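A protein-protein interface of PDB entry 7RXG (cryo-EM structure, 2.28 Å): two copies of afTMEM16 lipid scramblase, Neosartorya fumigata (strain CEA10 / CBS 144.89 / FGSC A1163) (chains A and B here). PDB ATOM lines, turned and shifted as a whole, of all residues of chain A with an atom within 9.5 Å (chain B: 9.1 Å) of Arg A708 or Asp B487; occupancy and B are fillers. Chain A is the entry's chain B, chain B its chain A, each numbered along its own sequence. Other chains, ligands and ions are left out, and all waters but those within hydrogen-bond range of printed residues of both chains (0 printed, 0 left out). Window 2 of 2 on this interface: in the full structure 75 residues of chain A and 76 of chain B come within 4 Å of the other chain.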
ATOM      1  N   PRO A 701     -13.866   2.463   0.626  1.00  0.00           N
ATOM      2  CA  PRO A 701     -14.753   2.437   1.793  1.00  0.00           C
ATOM      3  C   PRO A 701     -14.215   1.530   2.891  1.00  0.00           C
ATOM      4  O   PRO A 701     -13.994   1.976   4.019  1.00  0.00           O
ATOM      5  CB  PRO A 701     -16.073   1.891   1.229  1.00  0.00           C
ATOM      6  CG  PRO A 701     -15.937   1.966  -0.262  1.00  0.00           C
ATOM      7  CD  PRO A 701     -14.481   1.825  -0.545  1.00  0.00           C
ATOM      8  N   THR A 702     -14.009   0.257   2.544  1.00  0.00           N
ATOM      9  CA  THR A 702     -13.403  -0.683   3.478  1.00  0.00           C
ATOM     10  C   THR A 702     -11.895  -0.495   3.536  1.00  0.00           C
ATOM     11  O   THR A 702     -11.283  -0.666   4.592  1.00  0.00           O
ATOM     12  CB  THR A 702     -13.734  -2.120   3.082  1.00  0.00           C
ATOM     13  OG1 THR A 702     -12.976  -2.478   1.921  1.00  0.00           O
ATOM     14  CG2 THR A 702     -15.216  -2.260   2.777  1.00  0.00           C
ATOM     15  N   GLU A 703     -11.274  -0.162   2.409  1.00  0.00           N
ATOM     16  CA  GLU A 703      -9.836   0.053   2.398  1.00  0.00           C
ATOM     17  C   GLU A 703      -9.451   1.406   2.968  1.00  0.00           C
ATOM     18  O   GLU A 703      -8.303   1.580   3.383  1.00  0.00           O
ATOM     19  CB  GLU A 703      -9.285  -0.094   0.980  1.00  0.00           C
ATOM     20  CG  GLU A 703      -9.404  -1.504   0.438  1.00  0.00           C
ATOM     21  CD  GLU A 703      -8.570  -2.501   1.220  1.00  0.00           C
ATOM     22  OE1 GLU A 703      -7.495  -2.113   1.723  1.00  0.00           O
ATOM     23  OE2 GLU A 703      -8.993  -3.670   1.333  1.00  0.00           O
ATOM     24  N   ARG A 704     -10.381   2.361   3.011  1.00  0.00           N
ATOM     25  CA  ARG A 704     -10.121   3.610   3.710  1.00  0.00           C
ATOM     26  C   ARG A 704     -10.079   3.411   5.218  1.00  0.00           C
ATOM     27  O   ARG A 704      -9.463   4.215   5.922  1.00  0.00           O
ATOM     28  CB  ARG A 704     -11.178   4.649   3.339  1.00  0.00           C
ATOM     29  CG  ARG A 704     -11.255   4.930   1.847  1.00  0.00           C
ATOM     30  CD  ARG A 704     -12.128   6.135   1.547  1.00  0.00           C
ATOM     31  NE  ARG A 704     -13.523   5.901   1.903  1.00  0.00           N
ATOM     32  CZ  ARG A 704     -14.482   5.615   1.026  1.00  0.00           C
ATOM     33  NH1 ARG A 704     -15.723   5.419   1.442  1.00  0.00           N
ATOM     34  NH2 ARG A 704     -14.199   5.528  -0.267  1.00  0.00           N
ATOM     35  N   PHE A 705     -10.721   2.354   5.721  1.00  0.00           N
ATOM     36  CA  PHE A 705     -10.643   2.027   7.139  1.00  0.00           C
ATOM     37  C   PHE A 705      -9.215   1.679   7.541  1.00  0.00           C
ATOM     38  O   PHE A 705      -8.741   2.092   8.605  1.00  0.00           O
ATOM     39  CB  PHE A 705     -11.594   0.868   7.445  1.00  0.00           C
ATOM     40  CG  PHE A 705     -11.609   0.443   8.888  1.00  0.00           C
ATOM     41  CD1 PHE A 705     -12.415   1.088   9.804  1.00  0.00           C
ATOM     42  CD2 PHE A 705     -10.840  -0.619   9.320  1.00  0.00           C
ATOM     43  CE1 PHE A 705     -12.438   0.696  11.123  1.00  0.00           C
ATOM     44  CE2 PHE A 705     -10.859  -1.016  10.639  1.00  0.00           C
ATOM     45  CZ  PHE A 705     -11.659  -0.357  11.541  1.00  0.00           C
ATOM     46  N   TRP A 706      -8.514   0.934   6.698  1.00  0.00           N
ATOM     47  CA  TRP A 706      -7.181   0.451   7.008  1.00  0.00           C
ATOM     48  C   TRP A 706      -6.078   1.395   6.549  1.00  0.00           C
ATOM     49  O   TRP A 706      -4.905   1.135   6.828  1.00  0.00           O
ATOM     50  CB  TRP A 706      -6.986  -0.937   6.393  1.00  0.00           C
ATOM     51  CG  TRP A 706      -7.918  -1.952   6.976  1.00  0.00           C
ATOM     52  CD1 TRP A 706      -9.118  -2.347   6.472  1.00  0.00           C
ATOM     53  CD2 TRP A 706      -7.732  -2.683   8.189  1.00  0.00           C
ATOM     54  NE1 TRP A 706      -9.689  -3.287   7.292  1.00  0.00           N
ATOM     55  CE2 TRP A 706      -8.856  -3.511   8.354  1.00  0.00           C
ATOM     56  CE3 TRP A 706      -6.719  -2.726   9.148  1.00  0.00           C
ATOM     57  CZ2 TRP A 706      -8.998  -4.367   9.440  1.00  0.00           C
ATOM     58  CZ3 TRP A 706      -6.862  -3.572  10.223  1.00  0.00           C
ATOM     59  CH2 TRP A 706      -7.991  -4.382  10.361  1.00  0.00           C
ATOM     60  N   MET A 707      -6.422   2.486   5.873  1.00  0.00           N
ATOM     61  CA  MET A 707      -5.444   3.455   5.400  1.00  0.00           C
ATOM     62  C   MET A 707      -5.176   4.567   6.403  1.00  0.00           C
ATOM     63  O   MET A 707      -4.415   5.486   6.094  1.00  0.00           O
ATOM     64  CB  MET A 707      -5.913   4.062   4.074  1.00  0.00           C
ATOM     65  CG  MET A 707      -5.796   3.125   2.884  1.00  0.00           C
ATOM     66  SD  MET A 707      -6.676   3.725   1.425  1.00  0.00           S
ATOM     67  CE  MET A 707      -5.414   4.716   0.630  1.00  0.00           C
ATOM     68  N   ARG A 708      -5.777   4.506   7.591  1.00  0.00           N
ATOM     69  CA  ARG A 708      -5.671   5.606   8.543  1.00  0.00           C
ATOM     70  C   ARG A 708      -4.348   5.576   9.300  1.00  0.00           C
ATOM     71  O   ARG A 708      -3.733   6.623   9.530  1.00  0.00           O
ATOM     72  CB  ARG A 708      -6.842   5.558   9.523  1.00  0.00           C
ATOM     73  CG  ARG A 708      -8.155   5.177   8.881  1.00  0.00           C
ATOM     74  CD  ARG A 708      -8.921   6.406   8.446  1.00  0.00           C
ATOM     75  NE  ARG A 708      -9.550   7.078   9.577  1.00  0.00           N
ATOM     76  CZ  ARG A 708     -10.547   7.947   9.463  1.00  0.00           C
ATOM     77  NH1 ARG A 708     -11.064   8.514  10.544  1.00  0.00           N
ATOM     78  NH2 ARG A 708     -11.030   8.248   8.265  1.00  0.00           N
ATOM     79  N   GLN A 709      -3.903   4.390   9.702  1.00  0.00           N
ATOM     80  CA  GLN A 709      -2.685   4.223  10.484  1.00  0.00           C
ATOM     81  C   GLN A 709      -1.786   3.224   9.773  1.00  0.00           C
ATOM     82  O   GLN A 709      -2.152   2.054   9.623  1.00  0.00           O
ATOM     83  CB  GLN A 709      -3.017   3.765  11.904  1.00  0.00           C
ATOM     84  CG  GLN A 709      -4.097   4.607  12.567  1.00  0.00           C
ATOM     85  CD  GLN A 709      -4.811   3.883  13.687  1.00  0.00           C
ATOM     86  OE1 GLN A 709      -4.281   2.941  14.271  1.00  0.00           O
ATOM     87  NE2 GLN A 709      -6.021   4.324  13.996  1.00  0.00           N
ATOM     88  N   ARG A 710      -0.612   3.686   9.341  1.00  0.00           N
ATOM     89  CA  ARG A 710       0.230   2.899   8.445  1.00  0.00           C
ATOM     90  C   ARG A 710       0.844   1.697   9.154  1.00  0.00           C
ATOM     91  O   ARG A 710       0.595   0.548   8.776  1.00  0.00           O
ATOM     92  CB  ARG A 710       1.323   3.787   7.843  1.00  0.00           C
ATOM     93  N   GLY A 711       1.653   1.941  10.183  1.00  0.00           N
ATOM     94  CA  GLY A 711       2.303   0.890  10.924  1.00  0.00           C
ATOM     95  C   GLY A 711       1.888   0.859  12.382  1.00  0.00           C
ATOM     96  O   GLY A 711       0.975   1.559  12.820  1.00  0.00           O
ATOM     97  N   LYS A 713       3.293   2.057  14.861  1.00  0.00           N
ATOM     98  CA  LYS A 713       3.599   3.258  15.630  1.00  0.00           C
ATOM     99  C   LYS A 713       2.486   4.294  15.533  1.00  0.00           C
ATOM    100  O   LYS A 713       2.132   4.916  16.539  1.00  0.00           O
ATOM    101  CB  LYS A 713       4.936   3.850  15.180  1.00  0.00           C
ATOM    102  CG  LYS A 713       5.349   5.098  15.958  1.00  0.00           C
ATOM    103  CD  LYS A 713       5.558   4.786  17.438  1.00  0.00           C
ATOM    104  CE  LYS A 713       5.973   6.019  18.240  1.00  0.00           C
ATOM    105  NZ  LYS A 713       7.240   5.808  19.000  1.00  0.00           N
ATOM    106  N   GLU A 714       1.916   4.491  14.342  1.00  0.00           N
ATOM    107  CA  GLU A 714       0.799   5.422  14.214  1.00  0.00           C
ATOM    108  C   GLU A 714      -0.397   4.960  15.038  1.00  0.00           C
ATOM    109  O   GLU A 714      -1.077   5.777  15.672  1.00  0.00           O
ATOM    110  CB  GLU A 714       0.404   5.579  12.747  1.00  0.00           C
ATOM    111  CG  GLU A 714       1.380   6.384  11.910  1.00  0.00           C
ATOM    112  CD  GLU A 714       0.837   6.692  10.528  1.00  0.00           C
ATOM    113  OE1 GLU A 714       1.546   6.425   9.533  1.00  0.00           O
ATOM    114  OE2 GLU A 714      -0.300   7.201  10.437  1.00  0.00           O
ATOM    115  N   SER A 715      -0.670   3.654  15.047  1.00  0.00           N
ATOM    116  CA  SER A 715      -1.703   3.132  15.932  1.00  0.00           C
ATOM    117  C   SER A 715      -1.348   3.384  17.390  1.00  0.00           C
ATOM    118  O   SER A 715      -2.228   3.676  18.203  1.00  0.00           O
ATOM    119  CB  SER A 715      -1.912   1.639  15.684  1.00  0.00           C
ATOM    120  OG  SER A 715      -2.347   1.404  14.358  1.00  0.00           O
ATOM    121  N   GLU A 717       0.378   5.942  18.631  1.00  0.00           N
ATOM    122  CA  GLU A 717       0.118   7.337  18.970  1.00  0.00           C
ATOM    123  C   GLU A 717      -1.374   7.648  19.001  1.00  0.00           C
ATOM    124  O   GLU A 717      -1.814   8.445  19.835  1.00  0.00           O
ATOM    125  CB  GLU A 717       0.843   8.270  17.998  1.00  0.00           C
ATOM    126  CG  GLU A 717       0.451   8.117  16.538  1.00  0.00           C
ATOM    127  CD  GLU A 717       1.168   9.102  15.632  1.00  0.00           C
ATOM    128  OE1 GLU A 717       2.402   8.966  15.464  1.00  0.00           O
ATOM    129  OE2 GLU A 717       0.505  10.019  15.097  1.00  0.00           O
ATOM    130  N   VAL A 718      -2.167   7.030  18.118  1.00  0.00           N
ATOM    131  CA  VAL A 718      -3.617   7.188  18.200  1.00  0.00           C
ATOM    132  C   VAL A 718      -4.138   6.639  19.523  1.00  0.00           C
ATOM    133  O   VAL A 718      -5.007   7.244  20.164  1.00  0.00           O
ATOM    134  CB  VAL A 718      -4.296   6.512  16.996  1.00  0.00           C
ATOM    135  CG1 VAL A 718      -5.790   6.754  17.029  1.00  0.00           C
ATOM    136  CG2 VAL A 718      -3.725   7.046  15.709  1.00  0.00           C
ATOM    137  N   GLN B  49      -1.974  -6.672  10.560  1.00  0.00           N
ATOM    138  CA  GLN B  49      -2.174  -5.244  10.367  1.00  0.00           C
ATOM    139  C   GLN B  49      -3.209  -4.747  11.368  1.00  0.00           C
ATOM    140  O   GLN B  49      -4.249  -5.383  11.557  1.00  0.00           O
ATOM    141  CB  GLN B  49      -2.627  -4.954   8.938  1.00  0.00           C
ATOM    142  CG  GLN B  49      -3.006  -3.515   8.685  1.00  0.00           C
ATOM    143  CD  GLN B  49      -3.444  -3.279   7.259  1.00  0.00           C
ATOM    144  OE1 GLN B  49      -3.530  -4.210   6.462  1.00  0.00           O
ATOM    145  NE2 GLN B  49      -3.720  -2.027   6.925  1.00  0.00           N
ATOM    146  N   THR B  50      -2.923  -3.615  12.006  1.00  0.00           N
ATOM    147  CA  THR B  50      -3.745  -3.114  13.095  1.00  0.00           C
ATOM    148  C   THR B  50      -4.364  -1.770  12.746  1.00  0.00           C
ATOM    149  O   THR B  50      -3.789  -0.970  12.004  1.00  0.00           O
ATOM    150  CB  THR B  50      -2.935  -2.975  14.390  1.00  0.00           C
ATOM    151  OG1 THR B  50      -1.699  -2.308  14.116  1.00  0.00           O
ATOM    152  CG2 THR B  50      -2.643  -4.341  14.985  1.00  0.00           C
ATOM    153  N   GLU B  51      -5.558  -1.542  13.285  1.00  0.00           N
ATOM    154  CA  GLU B  51      -6.227  -0.250  13.259  1.00  0.00           C
ATOM    155  C   GLU B  51      -6.875  -0.046  14.616  1.00  0.00           C
ATOM    156  O   GLU B  51      -7.553  -0.945  15.119  1.00  0.00           O
ATOM    157  CB  GLU B  51      -7.285  -0.175  12.154  1.00  0.00           C
ATOM    158  CG  GLU B  51      -6.733   0.147  10.783  1.00  0.00           C
ATOM    159  CD  GLU B  51      -6.223   1.570  10.667  1.00  0.00           C
ATOM    160  OE1 GLU B  51      -6.749   2.456  11.371  1.00  0.00           O
ATOM    161  OE2 GLU B  51      -5.298   1.801   9.868  1.00  0.00           O
ATOM    162  N   VAL B  52      -6.669   1.125  15.206  1.00  0.00           N
ATOM    163  CA  VAL B  52      -7.102   1.409  16.567  1.00  0.00           C
ATOM    164  C   VAL B  52      -8.240   2.416  16.522  1.00  0.00           C
ATOM    165  O   VAL B  52      -8.122   3.468  15.884  1.00  0.00           O
ATOM    166  CB  VAL B  52      -5.939   1.931  17.424  1.00  0.00           C
ATOM    167  CG1 VAL B  52      -6.411   2.215  18.830  1.00  0.00           C
ATOM    168  CG2 VAL B  52      -4.801   0.926  17.432  1.00  0.00           C
ATOM    169  N   ARG B  53      -9.341   2.088  17.192  1.00  0.00           N
ATOM    170  CA  ARG B  53     -10.473   2.981  17.369  1.00  0.00           C
ATOM    171  C   ARG B  53     -10.913   2.934  18.824  1.00  0.00           C
ATOM    172  O   ARG B  53     -10.539   2.037  19.581  1.00  0.00           O
ATOM    173  CB  ARG B  53     -11.647   2.609  16.454  1.00  0.00           C
ATOM    174  CG  ARG B  53     -11.304   2.507  14.986  1.00  0.00           C
ATOM    175  CD  ARG B  53     -10.919   3.854  14.412  1.00  0.00           C
ATOM    176  NE  ARG B  53     -10.977   3.855  12.956  1.00  0.00           N
ATOM    177  CZ  ARG B  53      -9.974   3.490  12.169  1.00  0.00           C
ATOM    178  NH1 ARG B  53      -8.829   3.092  12.697  1.00  0.00           N
ATOM    179  NH2 ARG B  53     -10.115   3.522  10.854  1.00  0.00           N
ATOM    180  N   GLN B  54     -11.722   3.913  19.212  1.00  0.00           N
ATOM    181  CA  GLN B  54     -12.286   3.934  20.554  1.00  0.00           C
ATOM    182  C   GLN B  54     -13.387   2.888  20.665  1.00  0.00           C
ATOM    183  O   GLN B  54     -14.399   2.971  19.963  1.00  0.00           O
ATOM    184  CB  GLN B  54     -12.832   5.322  20.871  1.00  0.00           C
ATOM    185  CG  GLN B  54     -13.396   5.461  22.267  1.00  0.00           C
ATOM    186  CD  GLN B  54     -12.320   5.686  23.298  1.00  0.00           C
ATOM    187  OE1 GLN B  54     -11.298   6.305  23.017  1.00  0.00           O
ATOM    188  NE2 GLN B  54     -12.538   5.182  24.502  1.00  0.00           N
ATOM    189  N   ARG B  65      -6.049  -7.645  11.182  1.00  0.00           N
ATOM    190  CA  ARG B  65      -6.207  -8.228   9.863  1.00  0.00           C
ATOM    191  C   ARG B  65      -4.858  -8.768   9.417  1.00  0.00           C
ATOM    192  O   ARG B  65      -3.813  -8.260   9.825  1.00  0.00           O
ATOM    193  CB  ARG B  65      -6.736  -7.193   8.860  1.00  0.00           C
ATOM    194  CG  ARG B  65      -6.804  -7.674   7.432  1.00  0.00           C
ATOM    195  CD  ARG B  65      -7.521  -6.677   6.550  1.00  0.00           C
ATOM    196  NE  ARG B  65      -6.635  -5.628   6.062  1.00  0.00           N
ATOM    197  CZ  ARG B  65      -6.814  -4.983   4.915  1.00  0.00           C
ATOM    198  NH1 ARG B  65      -7.843  -5.284   4.138  1.00  0.00           N
ATOM    199  NH2 ARG B  65      -5.965  -4.038   4.543  1.00  0.00           N
ATOM    200  N   ASP B 487     -14.439   9.137  10.138  1.00  0.00           N
ATOM    201  CA  ASP B 487     -15.266   8.841  11.301  1.00  0.00           C
ATOM    202  C   ASP B 487     -16.745   8.827  10.939  1.00  0.00           C
ATOM    203  O   ASP B 487     -17.516   8.029  11.472  1.00  0.00           O
ATOM    204  CB  ASP B 487     -15.012   9.858  12.414  1.00  0.00           C
ATOM    205  CG  ASP B 487     -15.943   9.671  13.600  1.00  0.00           C
ATOM    206  OD1 ASP B 487     -16.351   8.521  13.868  1.00  0.00           O
ATOM    207  OD2 ASP B 487     -16.270  10.677  14.262  1.00  0.00           O
ATOM    208  N   GLU B 488     -17.144   9.720  10.035  1.00  0.00           N
ATOM    209  CA  GLU B 488     -18.542   9.793   9.633  1.00  0.00           C
ATOM    210  C   GLU B 488     -18.940   8.660   8.700  1.00  0.00           C
ATOM    211  O   GLU B 488     -20.127   8.331   8.620  1.00  0.00           O
ATOM    212  CB  GLU B 488     -18.830  11.140   8.967  1.00  0.00           C
ATOM    213  N   ASP B 489     -17.983   8.062   7.994  1.00  0.00           N
ATOM    214  CA  ASP B 489     -18.266   6.959   7.088  1.00  0.00           C
ATOM    215  C   ASP B 489     -18.126   5.593   7.749  1.00  0.00           C
ATOM    216  O   ASP B 489     -18.589   4.599   7.183  1.00  0.00           O
ATOM    217  CB  ASP B 489     -17.344   7.029   5.867  1.00  0.00           C
ATOM    218  N   GLU B 490     -17.504   5.519   8.926  1.00  0.00           N
ATOM    219  CA  GLU B 490     -17.386   4.278   9.678  1.00  0.00           C
ATOM    220  C   GLU B 490     -18.094   4.353  11.025  1.00  0.00           C
ATOM    221  O   GLU B 490     -17.796   3.563  11.924  1.00  0.00           O
ATOM    222  CB  GLU B 490     -15.914   3.912   9.872  1.00  0.00           C
ATOM    223  CG  GLU B 490     -15.206   4.725  10.934  1.00  0.00           C
ATOM    224  CD  GLU B 490     -13.702   4.716  10.764  1.00  0.00           C
ATOM    225  OE1 GLU B 490     -13.227   4.274   9.698  1.00  0.00           O
ATOM    226  OE2 GLU B 490     -12.995   5.150  11.696  1.00  0.00           O
ATOM    227  N   ALA B 491     -19.034   5.287  11.182  1.00  0.00           N
ATOM    228  CA  ALA B 491     -19.738   5.413  12.451  1.00  0.00           C
ATOM    229  C   ALA B 491     -20.766   4.307  12.639  1.00  0.00           C
ATOM    230  O   ALA B 491     -21.071   3.935  13.777  1.00  0.00           O
ATOM    231  CB  ALA B 491     -20.409   6.780  12.550  1.00  0.00           C
ATOM    232  N   ARG B 492     -21.310   3.771  11.548  1.00  0.00           N
ATOM    233  CA  ARG B 492     -22.258   2.670  11.665  1.00  0.00           C
ATOM    234  C   ARG B 492     -21.543   1.361  11.983  1.00  0.00           C
ATOM    235  O   ARG B 492     -21.944   0.633  12.899  1.00  0.00           O
ATOM    236  CB  ARG B 492     -23.076   2.537  10.382  1.00  0.00           C
ATOM    237  CG  ARG B 492     -24.054   1.381  10.408  1.00  0.00           C
ATOM    238  CD  ARG B 492     -24.951   1.375   9.185  1.00  0.00           C
ATOM    239  NE  ARG B 492     -24.187   1.467   7.945  1.00  0.00           N
ATOM    240  CZ  ARG B 492     -23.650   0.426   7.319  1.00  0.00           C
ATOM    241  NH1 ARG B 492     -23.787  -0.795   7.819  1.00  0.00           N
ATOM    242  NH2 ARG B 492     -22.972   0.604   6.194  1.00  0.00           N
ATOM    243  N   PHE B 493     -20.486   1.051  11.227  1.00  0.00           N
ATOM    244  CA  PHE B 493     -19.700  -0.150  11.490  1.00  0.00           C
ATOM    245  C   PHE B 493     -19.119  -0.129  12.897  1.00  0.00           C
ATOM    246  O   PHE B 493     -19.147  -1.141  13.603  1.00  0.00           O
ATOM    247  CB  PHE B 493     -18.589  -0.280  10.448  1.00  0.00           C
ATOM    248  CG  PHE B 493     -17.527  -1.279  10.803  1.00  0.00           C
ATOM    249  CD1 PHE B 493     -17.774  -2.636  10.714  1.00  0.00           C
ATOM    250  CD2 PHE B 493     -16.278  -0.860  11.214  1.00  0.00           C
ATOM    251  CE1 PHE B 493     -16.801  -3.552  11.034  1.00  0.00           C
ATOM    252  CE2 PHE B 493     -15.301  -1.772  11.537  1.00  0.00           C
ATOM    253  CZ  PHE B 493     -15.565  -3.123  11.446  1.00  0.00           C
ATOM    254  N   LEU B 494     -18.609   1.022  13.329  1.00  0.00           N
ATOM    255  CA  LEU B 494     -18.026   1.108  14.661  1.00  0.00           C
ATOM    256  C   LEU B 494     -19.081   0.972  15.748  1.00  0.00           C
ATOM    257  O   LEU B 494     -18.823   0.344  16.779  1.00  0.00           O
ATOM    258  CB  LEU B 494     -17.264   2.421  14.819  1.00  0.00           C
ATOM    259  CG  LEU B 494     -15.884   2.423  14.166  1.00  0.00           C
ATOM    260  CD1 LEU B 494     -15.110   3.670  14.541  1.00  0.00           C
ATOM    261  CD2 LEU B 494     -15.120   1.171  14.560  1.00  0.00           C
ATOM    262  N   THR B 495     -20.275   1.527  15.536  1.00  0.00           N
ATOM    263  CA  THR B 495     -21.319   1.375  16.541  1.00  0.00           C
ATOM    264  C   THR B 495     -21.818  -0.060  16.618  1.00  0.00           C
ATOM    265  O   THR B 495     -22.107  -0.554  17.713  1.00  0.00           O
ATOM    266  CB  THR B 495     -22.478   2.328  16.262  1.00  0.00           C
ATOM    267  OG1 THR B 495     -22.829   2.264  14.877  1.00  0.00           O
ATOM    268  CG2 THR B 495     -22.083   3.751  16.619  1.00  0.00           C
ATOM    269  N   ARG B 498     -19.205  -1.935  18.537  1.00  0.00           N
ATOM    270  CA  ARG B 498     -19.361  -1.654  19.959  1.00  0.00           C
ATOM    271  C   ARG B 498     -20.567  -2.379  20.543  1.00  0.00           C
ATOM    272  O   ARG B 498     -20.555  -2.748  21.722  1.00  0.00           O
ATOM    273  CB  ARG B 498     -19.481  -0.149  20.192  1.00  0.00           C
ATOM    274  CG  ARG B 498     -18.280   0.648  19.719  1.00  0.00           C
ATOM    275  CD  ARG B 498     -18.421   2.125  20.033  1.00  0.00           C
ATOM    276  NE  ARG B 498     -17.195   2.858  19.730  1.00  0.00           N
ATOM    277  CZ  ARG B 498     -17.052   3.680  18.696  1.00  0.00           C
ATOM    278  NH1 ARG B 498     -15.898   4.295  18.495  1.00  0.00           N
ATOM    279  NH2 ARG B 498     -18.062   3.889  17.865  1.00  0.00           N
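Of the 17 printed residues of chain B, 9 touch a printed residue of chain A.
Of the 16 printed residues of chain A, 6 touch a printed residue of chain B.
Among the printed residues, Asp or Glu carboxylates within 4 Å of a Lys or Arg side-chain nitrogen of the other chain: Glu A703 with Arg B65 (3.4 Å).
Phe A705 touches Glu B490 (CD1 to OE1, 3.3 Å).
Phe A705 touches Phe B493 (CE1 to CE2, 3.8 Å).
Trp A706 touches Thr B50.
Trp A706 touches Arg B65.
Arg A708 touches Glu B51 (N to OE2, 3.6 Å).
Arg A708 touches Arg B53.
Thr B50 touches Ser A715.
CG2 of Val B52 touches CB of Ser A715 (3.5 Å).
The guanidinium group of Arg B53 lies close to the side-chain amide nitrogen of Gln A709.
The backbone carbonyl oxygen (O) of Trp A706 is in hydrogen-bond range of the side-chain amide nitrogen (NE2) of Gln B49.
The backbone NH of Gln A709 is in hydrogen-bond range of the side-chain carboxylate of Glu B51, 2.9 Å away.
The side-chain carboxylate (OE2) of Glu A703 is in salt-bridge range of the guanidinium group (NH1) of Arg B65 (3.4 Å).
O of Phe A705 sits close to OE1 of Glu B51 (3.4 Å).
NH2 of Arg B53 lies within hydrogen-bond range of O of Phe A705, 3.0 Å away.
The side-chain carboxylate of Glu B51 sits close to the backbone carbonyl oxygen of Trp A706 (3.1 Å).
NH1 of Arg A708 sits close to N of Asp B487 (3.5 Å).
NE2 of Gln A709 lies within hydrogen-bond range of O of Val B52.
Of the printed residues of chain B, Gln A709 touches Glu B51, Val B52 and Arg B53.
Of the printed residues of chain A, Thr B50 touches Trp A706 and Ser A715.
Printed residues of chain A within 4 Å of Glu B51: Phe A705 (3.3 Å), Trp A706 (3.1 Å), Arg A708 (3.6 Å) and Gln A709 (2.9 Å).
Of the printed residues of chain A, Arg B53 touches Phe A705, Arg A708 and Gln A709.
Printed residues of chain A within 4 Å of Asp B487: Arg A708 (3.5 Å).
No residue of chain A comes within 4 Å of Glu B488.
Printed residues of chain A within 4 Å of Phe B493: Phe A705 (3.8 Å).
The nearest residue of chain A that does not touch Asp B487 is Arg A704 (8.2 Å).
No position is printed for both chains.
Of the 17 pairs that touch across the chains among the printed residues, none has its exchanged pair printed and touching as well.
The side-chain amide oxygen of Gln A709 lies within hydrogen-bond range of the side-chain hydroxyl of Ser A715 (2.5 Å).
The backbone carbonyl oxygen (O) of Arg B65 is in hydrogen-bond range of the backbone NH (N) of Gln B49 (2.5 Å).
NE of Arg B53 lies within salt-bridge range of OE2 of Glu B490 (2.7 Å).
OE1 of Glu B51 lies within salt-bridge range of NH1 of Arg B53.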
